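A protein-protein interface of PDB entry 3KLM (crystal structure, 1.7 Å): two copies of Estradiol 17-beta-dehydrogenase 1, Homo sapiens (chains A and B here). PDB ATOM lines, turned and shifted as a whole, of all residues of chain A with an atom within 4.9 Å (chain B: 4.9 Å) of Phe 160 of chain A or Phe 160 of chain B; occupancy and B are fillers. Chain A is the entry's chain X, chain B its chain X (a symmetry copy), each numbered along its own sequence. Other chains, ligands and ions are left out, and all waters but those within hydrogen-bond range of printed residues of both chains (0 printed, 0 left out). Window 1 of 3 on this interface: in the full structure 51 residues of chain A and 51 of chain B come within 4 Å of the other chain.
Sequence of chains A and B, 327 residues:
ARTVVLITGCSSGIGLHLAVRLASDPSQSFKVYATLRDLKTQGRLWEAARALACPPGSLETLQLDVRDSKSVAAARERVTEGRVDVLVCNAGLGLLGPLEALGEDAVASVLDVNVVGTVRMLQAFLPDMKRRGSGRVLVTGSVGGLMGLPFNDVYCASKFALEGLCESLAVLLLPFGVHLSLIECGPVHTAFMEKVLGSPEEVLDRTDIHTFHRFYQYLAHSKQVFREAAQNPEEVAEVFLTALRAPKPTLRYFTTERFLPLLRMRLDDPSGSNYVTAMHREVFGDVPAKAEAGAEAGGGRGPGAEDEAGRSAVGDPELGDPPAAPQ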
ATOM      1  N   GLY A 144       2.883 -28.490  17.167  1.00  0.00           N
ATOM      2  CA  GLY A 144       3.967 -27.581  17.674  1.00  0.00           C
ATOM      3  C   GLY A 144       3.426 -26.494  18.639  1.00  0.00           C
ATOM      4  O   GLY A 144       4.200 -25.738  19.218  1.00  0.00           O
ATOM      5  N   GLY A 145       2.108 -26.393  18.771  1.00  0.00           N
ATOM      6  CA  GLY A 145       1.521 -25.586  19.812  1.00  0.00           C
ATOM      7  C   GLY A 145       1.356 -26.299  21.131  1.00  0.00           C
ATOM      8  O   GLY A 145       1.062 -25.675  22.134  1.00  0.00           O
ATOM      9  N   LEU A 146       1.482 -27.641  21.073  1.00  0.00           N
ATOM     10  CA  LEU A 146       1.227 -28.515  22.210  1.00  0.00           C
ATOM     11  C   LEU A 146       2.489 -29.137  22.809  1.00  0.00           C
ATOM     12  O   LEU A 146       2.466 -29.603  23.973  1.00  0.00           O
ATOM     13  CB  LEU A 146       0.329 -29.655  21.738  1.00  0.00           C
ATOM     14  CG  LEU A 146      -1.023 -29.320  21.093  1.00  0.00           C
ATOM     15  CD1 LEU A 146      -1.703 -30.603  20.630  1.00  0.00           C
ATOM     16  CD2 LEU A 146      -1.847 -28.602  22.112  1.00  0.00           C
ATOM     17  N   MET A 147       3.551 -29.146  22.031  1.00  0.00           N
ATOM     18  CA  MET A 147       4.846 -29.666  22.486  1.00  0.00           C
ATOM     19  C   MET A 147       5.934 -28.998  21.679  1.00  0.00           C
ATOM     20  O   MET A 147       5.758 -28.737  20.472  1.00  0.00           O
ATOM     21  CB  MET A 147       4.852 -31.235  22.324  1.00  0.00           C
ATOM     22  CG  MET A 147       4.754 -31.644  20.878  1.00  0.00           C
ATOM     23  SD  MET A 147       4.477 -33.447  20.664  1.00  0.00           S
ATOM     24  CE  MET A 147       2.843 -33.576  21.264  1.00  0.00           C
ATOM     25  N   GLY A 148       7.072 -28.723  22.326  1.00  0.00           N
ATOM     26  CA  GLY A 148       8.187 -28.052  21.669  1.00  0.00           C
ATOM     27  C   GLY A 148       8.923 -28.943  20.667  1.00  0.00           C
ATOM     28  O   GLY A 148       9.135 -30.108  20.929  1.00  0.00           O
ATOM     29  N   CYS A 156       6.978 -22.653  17.342  1.00  0.00           N
ATOM     30  CA  CYS A 156       6.352 -23.255  18.558  1.00  0.00           C
ATOM     31  C   CYS A 156       5.974 -22.134  19.549  1.00  0.00           C
ATOM     32  O   CYS A 156       4.874 -22.150  20.133  1.00  0.00           O
ATOM     33  CB  CYS A 156       7.340 -24.217  19.190  1.00  0.00           C
ATOM     34  SG  CYS A 156       7.434 -25.790  18.263  1.00  0.00           S
ATOM     35  N   ALA A 157       6.848 -21.156  19.774  1.00  0.00           N
ATOM     36  CA  ALA A 157       6.443 -20.059  20.640  1.00  0.00           C
ATOM     37  C   ALA A 157       5.117 -19.476  20.179  1.00  0.00           C
ATOM     38  O   ALA A 157       4.179 -19.234  20.970  1.00  0.00           O
ATOM     39  CB  ALA A 157       7.561 -18.980  20.695  1.00  0.00           C
ATOM     40  N   SER A 158       4.998 -19.234  18.893  1.00  0.00           N
ATOM     41  CA  SER A 158       3.801 -18.608  18.346  1.00  0.00           C
ATOM     42  C   SER A 158       2.530 -19.478  18.454  1.00  0.00           C
ATOM     43  O   SER A 158       1.410 -18.984  18.716  1.00  0.00           O
ATOM     44  CB  SER A 158       4.078 -18.210  16.859  1.00  0.00           C
ATOM     45  OG  SER A 158       3.910 -19.275  15.965  1.00  0.00           O
ATOM     46  N   LYS A 159       2.674 -20.800  18.228  1.00  0.00           N
ATOM     47  CA  LYS A 159       1.597 -21.751  18.312  1.00  0.00           C
ATOM     48  C   LYS A 159       1.178 -22.097  19.816  1.00  0.00           C
ATOM     49  O   LYS A 159       0.001 -22.081  20.120  1.00  0.00           O
ATOM     50  CB  LYS A 159       1.935 -23.003  17.502  1.00  0.00           C
ATOM     51  CG  LYS A 159       1.985 -22.762  15.915  1.00  0.00           C
ATOM     52  CD  LYS A 159       0.511 -22.563  15.410  1.00  0.00           C
ATOM     53  CE  LYS A 159       0.341 -21.812  14.041  1.00  0.00           C
ATOM     54  NZ  LYS A 159      -1.093 -22.103  13.587  1.00  0.00           N
ATOM     55  N   PHE A 160       2.133 -22.181  20.717  1.00  0.00           N
ATOM     56  CA  PHE A 160       1.864 -22.160  22.153  1.00  0.00           C
ATOM     57  C   PHE A 160       1.130 -20.888  22.535  1.00  0.00           C
ATOM     58  O   PHE A 160       0.217 -20.910  23.311  1.00  0.00           O
ATOM     59  CB  PHE A 160       3.139 -22.239  22.977  1.00  0.00           C
ATOM     60  CG  PHE A 160       3.675 -23.683  23.237  1.00  0.00           C
ATOM     61  CD1 PHE A 160       4.167 -24.453  22.202  1.00  0.00           C
ATOM     62  CD2 PHE A 160       3.732 -24.173  24.540  1.00  0.00           C
ATOM     63  CE1 PHE A 160       4.712 -25.743  22.457  1.00  0.00           C
ATOM     64  CE2 PHE A 160       4.264 -25.426  24.833  1.00  0.00           C
ATOM     65  CZ  PHE A 160       4.708 -26.215  23.791  1.00  0.00           C
ATOM     66  N   ALA A 161       1.540 -19.745  21.973  1.00  0.00           N
ATOM     67  CA  ALA A 161       0.824 -18.485  22.310  1.00  0.00           C
ATOM     68  C   ALA A 161      -0.660 -18.494  21.957  1.00  0.00           C
ATOM     69  O   ALA A 161      -1.468 -17.967  22.727  1.00  0.00           O
ATOM     70  CB  ALA A 161       1.538 -17.286  21.644  1.00  0.00           C
ATOM     71  N   LEU A 162      -1.014 -19.101  20.820  1.00  0.00           N
ATOM     72  CA  LEU A 162      -2.402 -19.202  20.359  1.00  0.00           C
ATOM     73  C   LEU A 162      -3.138 -20.092  21.359  1.00  0.00           C
ATOM     74  O   LEU A 162      -4.325 -19.863  21.665  1.00  0.00           O
ATOM     75  CB  LEU A 162      -2.514 -19.786  18.901  1.00  0.00           C
ATOM     76  CG  LEU A 162      -2.289 -18.815  17.746  1.00  0.00           C
ATOM     77  CD1 LEU A 162      -2.414 -19.538  16.389  1.00  0.00           C
ATOM     78  CD2 LEU A 162      -3.376 -17.813  17.858  1.00  0.00           C
ATOM     79  N   GLU A 163      -2.447 -21.104  21.894  1.00  0.00           N
ATOM     80  CA  GLU A 163      -3.131 -21.933  22.871  1.00  0.00           C
ATOM     81  C   GLU A 163      -3.535 -21.087  24.099  1.00  0.00           C
ATOM     82  O   GLU A 163      -4.695 -21.160  24.580  1.00  0.00           O
ATOM     83  CB  GLU A 163      -2.278 -23.129  23.331  1.00  0.00           C
ATOM     84  CG  GLU A 163      -1.913 -24.135  22.249  1.00  0.00           C
ATOM     85  CD  GLU A 163      -3.076 -25.015  21.849  1.00  0.00           C
ATOM     86  OE1 GLU A 163      -3.730 -25.556  22.758  1.00  0.00           O
ATOM     87  OE2 GLU A 163      -3.315 -25.201  20.646  1.00  0.00           O
ATOM     88  N   GLY A 164      -2.576 -20.361  24.680  1.00  0.00           N
ATOM     89  CA  GLY A 164      -2.860 -19.552  25.855  1.00  0.00           C
ATOM     90  C   GLY A 164      -3.893 -18.505  25.527  1.00  0.00           C
ATOM     91  O   GLY A 164      -4.747 -18.249  26.349  1.00  0.00           O
ATOM     92  N   GLU A 167      -7.386 -20.293  25.145  1.00  0.00           N
ATOM     93  CA  GLU A 167      -7.882 -20.920  26.363  1.00  0.00           C
ATOM     94  C   GLU A 167      -8.364 -19.850  27.340  1.00  0.00           C
ATOM     95  O   GLU A 167      -9.422 -19.947  27.943  1.00  0.00           O
ATOM     96  CB  GLU A 167      -6.780 -21.732  27.001  1.00  0.00           C
ATOM     97  CG  GLU A 167      -7.190 -22.726  28.093  1.00  0.00           C
ATOM     98  CD  GLU A 167      -6.055 -23.687  28.336  1.00  0.00           C
ATOM     99  OE1 GLU A 167      -5.328 -23.489  29.333  1.00  0.00           O
ATOM    100  OE2 GLU A 167      -5.906 -24.669  27.562  1.00  0.00           O
ATOM    101  N   ARG A 266       4.208 -35.988  27.630  1.00  0.00           N
ATOM    102  CA  ARG A 266       4.437 -34.600  28.029  1.00  0.00           C
ATOM    103  C   ARG A 266       3.514 -34.239  29.186  1.00  0.00           C
ATOM    104  O   ARG A 266       3.926 -33.714  30.223  1.00  0.00           O
ATOM    105  CB  ARG A 266       4.123 -33.670  26.859  1.00  0.00           C
ATOM    106  CG  ARG A 266       4.425 -32.233  27.189  1.00  0.00           C
ATOM    107  CD  ARG A 266       4.170 -31.293  25.980  1.00  0.00           C
ATOM    108  NE  ARG A 266       4.655 -29.971  26.381  1.00  0.00           N
ATOM    109  CZ  ARG A 266       4.011 -29.096  27.156  1.00  0.00           C
ATOM    110  NH1 ARG A 266       2.733 -29.318  27.557  1.00  0.00           N
ATOM    111  NH2 ARG A 266       4.617 -27.942  27.522  1.00  0.00           N
ATOM    112  N   GLY B 144       0.254 -18.703  34.554  1.00  0.00           N
ATOM    113  CA  GLY B 144      -0.439 -18.208  33.315  1.00  0.00           C
ATOM    114  C   GLY B 144       0.282 -18.652  32.015  1.00  0.00           C
ATOM    115  O   GLY B 144      -0.216 -18.413  30.919  1.00  0.00           O
ATOM    116  N   GLY B 145       1.461 -19.249  32.142  1.00  0.00           N
ATOM    117  CA  GLY B 145       2.090 -19.906  31.023  1.00  0.00           C
ATOM    118  C   GLY B 145       1.657 -21.337  30.821  1.00  0.00           C
ATOM    119  O   GLY B 145       1.959 -21.932  29.802  1.00  0.00           O
ATOM    120  N   LEU B 146       1.003 -21.888  31.864  1.00  0.00           N
ATOM    121  CA  LEU B 146       0.623 -23.293  31.914  1.00  0.00           C
ATOM    122  C   LEU B 146      -0.880 -23.535  31.764  1.00  0.00           C
ATOM    123  O   LEU B 146      -1.302 -24.668  31.434  1.00  0.00           O
ATOM    124  CB  LEU B 146       1.048 -23.850  33.270  1.00  0.00           C
ATOM    125  CG  LEU B 146       2.521 -23.749  33.687  1.00  0.00           C
ATOM    126  CD1 LEU B 146       2.692 -24.292  35.101  1.00  0.00           C
ATOM    127  CD2 LEU B 146       3.328 -24.530  32.701  1.00  0.00           C
ATOM    128  N   MET B 147      -1.656 -22.499  32.008  1.00  0.00           N
ATOM    129  CA  MET B 147      -3.114 -22.566  31.859  1.00  0.00           C
ATOM    130  C   MET B 147      -3.627 -21.171  31.591  1.00  0.00           C
ATOM    131  O   MET B 147      -3.104 -20.186  32.150  1.00  0.00           O
ATOM    132  CB  MET B 147      -3.733 -23.197  33.166  1.00  0.00           C
ATOM    133  CG  MET B 147      -3.504 -22.318  34.367  1.00  0.00           C
ATOM    134  SD  MET B 147      -3.958 -23.137  35.947  1.00  0.00           S
ATOM    135  CE  MET B 147      -2.695 -24.338  36.039  1.00  0.00           C
ATOM    136  N   GLY B 148      -4.659 -21.068  30.747  1.00  0.00           N
ATOM    137  CA  GLY B 148      -5.227 -19.775  30.382  1.00  0.00           C
ATOM    138  C   GLY B 148      -6.031 -19.128  31.510  1.00  0.00           C
ATOM    139  O   GLY B 148      -6.756 -19.805  32.208  1.00  0.00           O
ATOM    140  N   CYS B 156      -0.995 -14.328  29.060  1.00  0.00           N
ATOM    141  CA  CYS B 156      -0.951 -15.816  28.933  1.00  0.00           C
ATOM    142  C   CYS B 156      -0.367 -16.196  27.557  1.00  0.00           C
ATOM    143  O   CYS B 156       0.474 -17.110  27.457  1.00  0.00           O
ATOM    144  CB  CYS B 156      -2.360 -16.360  29.086  1.00  0.00           C
ATOM    145  SG  CYS B 156      -2.893 -16.365  30.834  1.00  0.00           S
ATOM    146  N   ALA B 157      -0.785 -15.537  26.479  1.00  0.00           N
ATOM    147  CA  ALA B 157      -0.159 -15.843  25.201  1.00  0.00           C
ATOM    148  C   ALA B 157       1.354 -15.755  25.312  1.00  0.00           C
ATOM    149  O   ALA B 157       2.114 -16.636  24.854  1.00  0.00           O
ATOM    150  CB  ALA B 157      -0.714 -14.903  24.094  1.00  0.00           C
ATOM    151  N   SER B 158       1.837 -14.693  25.919  1.00  0.00           N
ATOM    152  CA  SER B 158       3.272 -14.464  26.021  1.00  0.00           C
ATOM    153  C   SER B 158       4.014 -15.493  26.902  1.00  0.00           C
ATOM    154  O   SER B 158       5.152 -15.920  26.604  1.00  0.00           O
ATOM    155  CB  SER B 158       3.511 -13.009  26.543  1.00  0.00           C
ATOM    156  OG  SER B 158       3.412 -12.903  27.936  1.00  0.00           O
ATOM    157  N   LYS B 159       3.388 -15.896  28.026  1.00  0.00           N
ATOM    158  CA  LYS B 159       3.931 -16.865  28.943  1.00  0.00           C
ATOM    159  C   LYS B 159       3.835 -18.367  28.400  1.00  0.00           C
ATOM    160  O   LYS B 159       4.817 -19.081  28.459  1.00  0.00           O
ATOM    161  CB  LYS B 159       3.288 -16.705  30.321  1.00  0.00           C
ATOM    162  CG  LYS B 159       3.684 -15.343  31.073  1.00  0.00           C
ATOM    163  CD  LYS B 159       5.180 -15.466  31.538  1.00  0.00           C
ATOM    164  CE  LYS B 159       5.935 -14.116  31.814  1.00  0.00           C
ATOM    165  NZ  LYS B 159       7.182 -14.499  32.618  1.00  0.00           N
ATOM    166  N   PHE B 160       2.761 -18.708  27.721  1.00  0.00           N
ATOM    167  CA  PHE B 160       2.698 -19.918  26.904  1.00  0.00           C
ATOM    168  C   PHE B 160       3.791 -19.903  25.852  1.00  0.00           C
ATOM    169  O   PHE B 160       4.423 -20.890  25.602  1.00  0.00           O
ATOM    170  CB  PHE B 160       1.360 -20.066  26.198  1.00  0.00           C
ATOM    171  CG  PHE B 160       0.233 -20.742  27.042  1.00  0.00           C
ATOM    172  CD1 PHE B 160      -0.298 -20.111  28.150  1.00  0.00           C
ATOM    173  CD2 PHE B 160      -0.300 -21.962  26.629  1.00  0.00           C
ATOM    174  CE1 PHE B 160      -1.368 -20.705  28.876  1.00  0.00           C
ATOM    175  CE2 PHE B 160      -1.352 -22.572  27.307  1.00  0.00           C
ATOM    176  CZ  PHE B 160      -1.847 -21.965  28.444  1.00  0.00           C
ATOM    177  N   ALA B 161       4.022 -18.748  25.216  1.00  0.00           N
ATOM    178  CA  ALA B 161       5.104 -18.695  24.197  1.00  0.00           C
ATOM    179  C   ALA B 161       6.488 -19.040  24.734  1.00  0.00           C
ATOM    180  O   ALA B 161       7.256 -19.714  24.041  1.00  0.00           O
ATOM    181  CB  ALA B 161       5.110 -17.307  23.516  1.00  0.00           C
ATOM    182  N   LEU B 162       6.796 -18.602  25.959  1.00  0.00           N
ATOM    183  CA  LEU B 162       8.081 -18.868  26.611  1.00  0.00           C
ATOM    184  C   LEU B 162       8.150 -20.374  26.859  1.00  0.00           C
ATOM    185  O   LEU B 162       9.229 -20.990  26.755  1.00  0.00           O
ATOM    186  CB  LEU B 162       8.253 -18.071  27.958  1.00  0.00           C
ATOM    187  CG  LEU B 162       8.703 -16.617  27.850  1.00  0.00           C
ATOM    188  CD1 LEU B 162       8.807 -15.970  29.247  1.00  0.00           C
ATOM    189  CD2 LEU B 162      10.056 -16.670  27.244  1.00  0.00           C
ATOM    190  N   GLU B 163       7.004 -20.990  27.172  1.00  0.00           N
ATOM    191  CA  GLU B 163       7.057 -22.427  27.375  1.00  0.00           C
ATOM    192  C   GLU B 163       7.500 -23.135  26.074  1.00  0.00           C
ATOM    193  O   GLU B 163       8.393 -24.021  26.093  1.00  0.00           O
ATOM    194  CB  GLU B 163       5.709 -23.007  27.840  1.00  0.00           C
ATOM    195  CG  GLU B 163       5.203 -22.506  29.185  1.00  0.00           C
ATOM    196  CD  GLU B 163       5.954 -23.103  30.354  1.00  0.00           C
ATOM    197  OE1 GLU B 163       6.114 -24.337  30.368  1.00  0.00           O
ATOM    198  OE2 GLU B 163       6.348 -22.363  31.268  1.00  0.00           O
ATOM    199  N   GLY B 164       6.827 -22.836  24.959  1.00  0.00           N
ATOM    200  CA  GLY B 164       7.159 -23.471  23.694  1.00  0.00           C
ATOM    201  C   GLY B 164       8.576 -23.139  23.303  1.00  0.00           C
ATOM    202  O   GLY B 164       9.261 -24.003  22.798  1.00  0.00           O
ATOM    203  N   GLU B 167      11.010 -25.150  25.664  1.00  0.00           N
ATOM    204  CA  GLU B 167      10.928 -26.599  25.528  1.00  0.00           C
ATOM    205  C   GLU B 167      11.586 -27.035  24.220  1.00  0.00           C
ATOM    206  O   GLU B 167      12.353 -27.986  24.162  1.00  0.00           O
ATOM    207  CB  GLU B 167       9.480 -27.027  25.535  1.00  0.00           C
ATOM    208  CG  GLU B 167       9.197 -28.520  25.738  1.00  0.00           C
ATOM    209  CD  GLU B 167       7.743 -28.702  26.090  1.00  0.00           C
ATOM    210  OE1 GLU B 167       6.967 -29.076  25.185  1.00  0.00           O
ATOM    211  OE2 GLU B 167       7.372 -28.517  27.280  1.00  0.00           O
ATOM    212  N   ARG B 266      -6.270 -29.853  33.802  1.00  0.00           N
ATOM    213  CA  ARG B 266      -5.984 -29.397  32.443  1.00  0.00           C
ATOM    214  C   ARG B 266      -5.268 -30.497  31.670  1.00  0.00           C
ATOM    215  O   ARG B 266      -5.638 -30.874  30.556  1.00  0.00           O
ATOM    216  CB  ARG B 266      -5.071 -28.174  32.492  1.00  0.00           C
ATOM    217  CG  ARG B 266      -4.815 -27.611  31.120  1.00  0.00           C
ATOM    218  CD  ARG B 266      -3.940 -26.329  31.171  1.00  0.00           C
ATOM    219  NE  ARG B 266      -3.910 -25.800  29.807  1.00  0.00           N
ATOM    220  CZ  ARG B 266      -3.145 -26.241  28.806  1.00  0.00           C
ATOM    221  NH1 ARG B 266      -2.192 -27.187  29.012  1.00  0.00           N
ATOM    222  NH2 ARG B 266      -3.283 -25.718  27.566  1.00  0.00           N
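The side-chain carboxylate (OE1) of Glu 167 of chain A lies within salt-bridge range of the guanidinium group (NE) of Arg 266 of chain B. The guanidinium group (NE) of Arg 266 of chain A lies within salt-bridge range of the side-chain carboxylate (OE1) of Glu 167 of chain B (2.8 Å). The backbone NH (N) of Gly 148 of chain A lies within hydrogen-bond range of the side-chain carboxylate (OE1) of Glu 167 of chain B, at 2.9 Å. OE1 of Glu 167 of chain A is in hydrogen-bond range of N of Gly 148 of chain B, 2.9 Å away.
O of Leu 146 of chain B sits close to NE of Arg 266 of chain B. The backbone carbonyl oxygen (O) of Leu 146 of chain A sits close to the guanidinium group (NE) of Arg 266 of chain A, at 3.3 Å.
Met 147 of chain A touches Glu 167 of chain B (CA to OE1, 3.5 Å). Ala 157 of chain A touches Ala 161 of chain B (O to CB, 3.3 Å). Phe 160 of chain B touches Phe 160 of chain A. N of Gly 164 of chain B touches CD2 of Phe 160 of chain A, 3.4 Å away. Glu 167 of chain B touches Phe 160 of chain A (OE1 to CZ, 3.9 Å). O of Ala 157 of chain B touches CB of Ala 161 of chain A (3.3 Å). Gly 164 of chain A touches Phe 160 of chain B. OE1 of Glu 167 of chain A touches CA of Met 147 of chain B, 3.5 Å away. Glu 167 of chain A touches Phe 160 of chain B (OE1 to CZ, 3.9 Å).
Printed residues of chain B within 4 Å of Phe 160 of chain A: Phe 160, Gly 164 and Glu 167. Printed residues of chain B within 4 Å of Gly 164 of chain A: Phe 160 (3.4 Å). Of the printed residues of chain B, Arg 266 of chain A touches Glu 167. Leu 146 of chain B touches none of the printed residues of chain A. Printed residues of chain A within 4 Å of Gly 148 of chain B: Glu 167. Leu 162 of chain B touches none of the printed residues of chain A. Printed residues of chain A within 4 Å of Gly 164 of chain B: Phe 160 (3.4 Å). Of the printed residues of chain A, Glu 167 of chain B touches Met 147 (3.5 Å), Gly 148 (2.9 Å), Phe 160 (3.9 Å) and Arg 266 (2.8 Å). The nearest printed residue of chain B that does not touch Phe 160 of chain A is Glu 163 of chain B (4.02 Å). The nearest printed residue of chain A that does not touch Phe 160 of chain B is Glu 163 of chain A (4.02 Å). The nearest printed residue of chain A that does not touch Ala 157 of chain B is Gly 164 of chain A (4.4 Å).
Hydrophobic or aromatic side chains of chain B within 4 Å of the printed part of chain A: Ala 157, Phe 160 and Ala 161. Along chain B the printed residues that touch a printed residue of chain A span positions 147 to 266. Printed residues of chain A that touch a printed residue of chain B: Met 147, Gly 148, Ala 157, Phe 160, Ala 161, Gly 164, Glu 167 and Arg 266. Hydrophobic or aromatic side chains of chain A that line the printed part of chain B: Ala 157, Phe 160 and Ala 161. Along chain A the printed residues that touch a printed residue of chain B span positions 147 to 266. Among the printed residues, 13 pairs touch across the chains. Among the printed residues, Asp or Glu carboxylates within 4 Å of a Lys or Arg side-chain nitrogen of the other chain: Glu 167 of chain A with Arg 266 of chain B (2.8 Å) and Arg 266 of chain A with Glu 167 of chain B (2.8 Å).
Gly 148 of chain A touches Glu 167 of chain B, and with the chains exchanged Glu 167 of chain A touches Gly 148 of chain B. Phe 160 of chain A touches its own counterpart, Phe 160 of chain B. Phe 160 of chain A touches Glu 167 of chain B, and with the chains exchanged Glu 167 of chain A touches Phe 160 of chain B. Glu 167 of chain A touches Arg 266 of chain B, and with the chains exchanged Arg 266 of chain A touches Glu 167 of chain B. 16 positions are printed for both chains.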
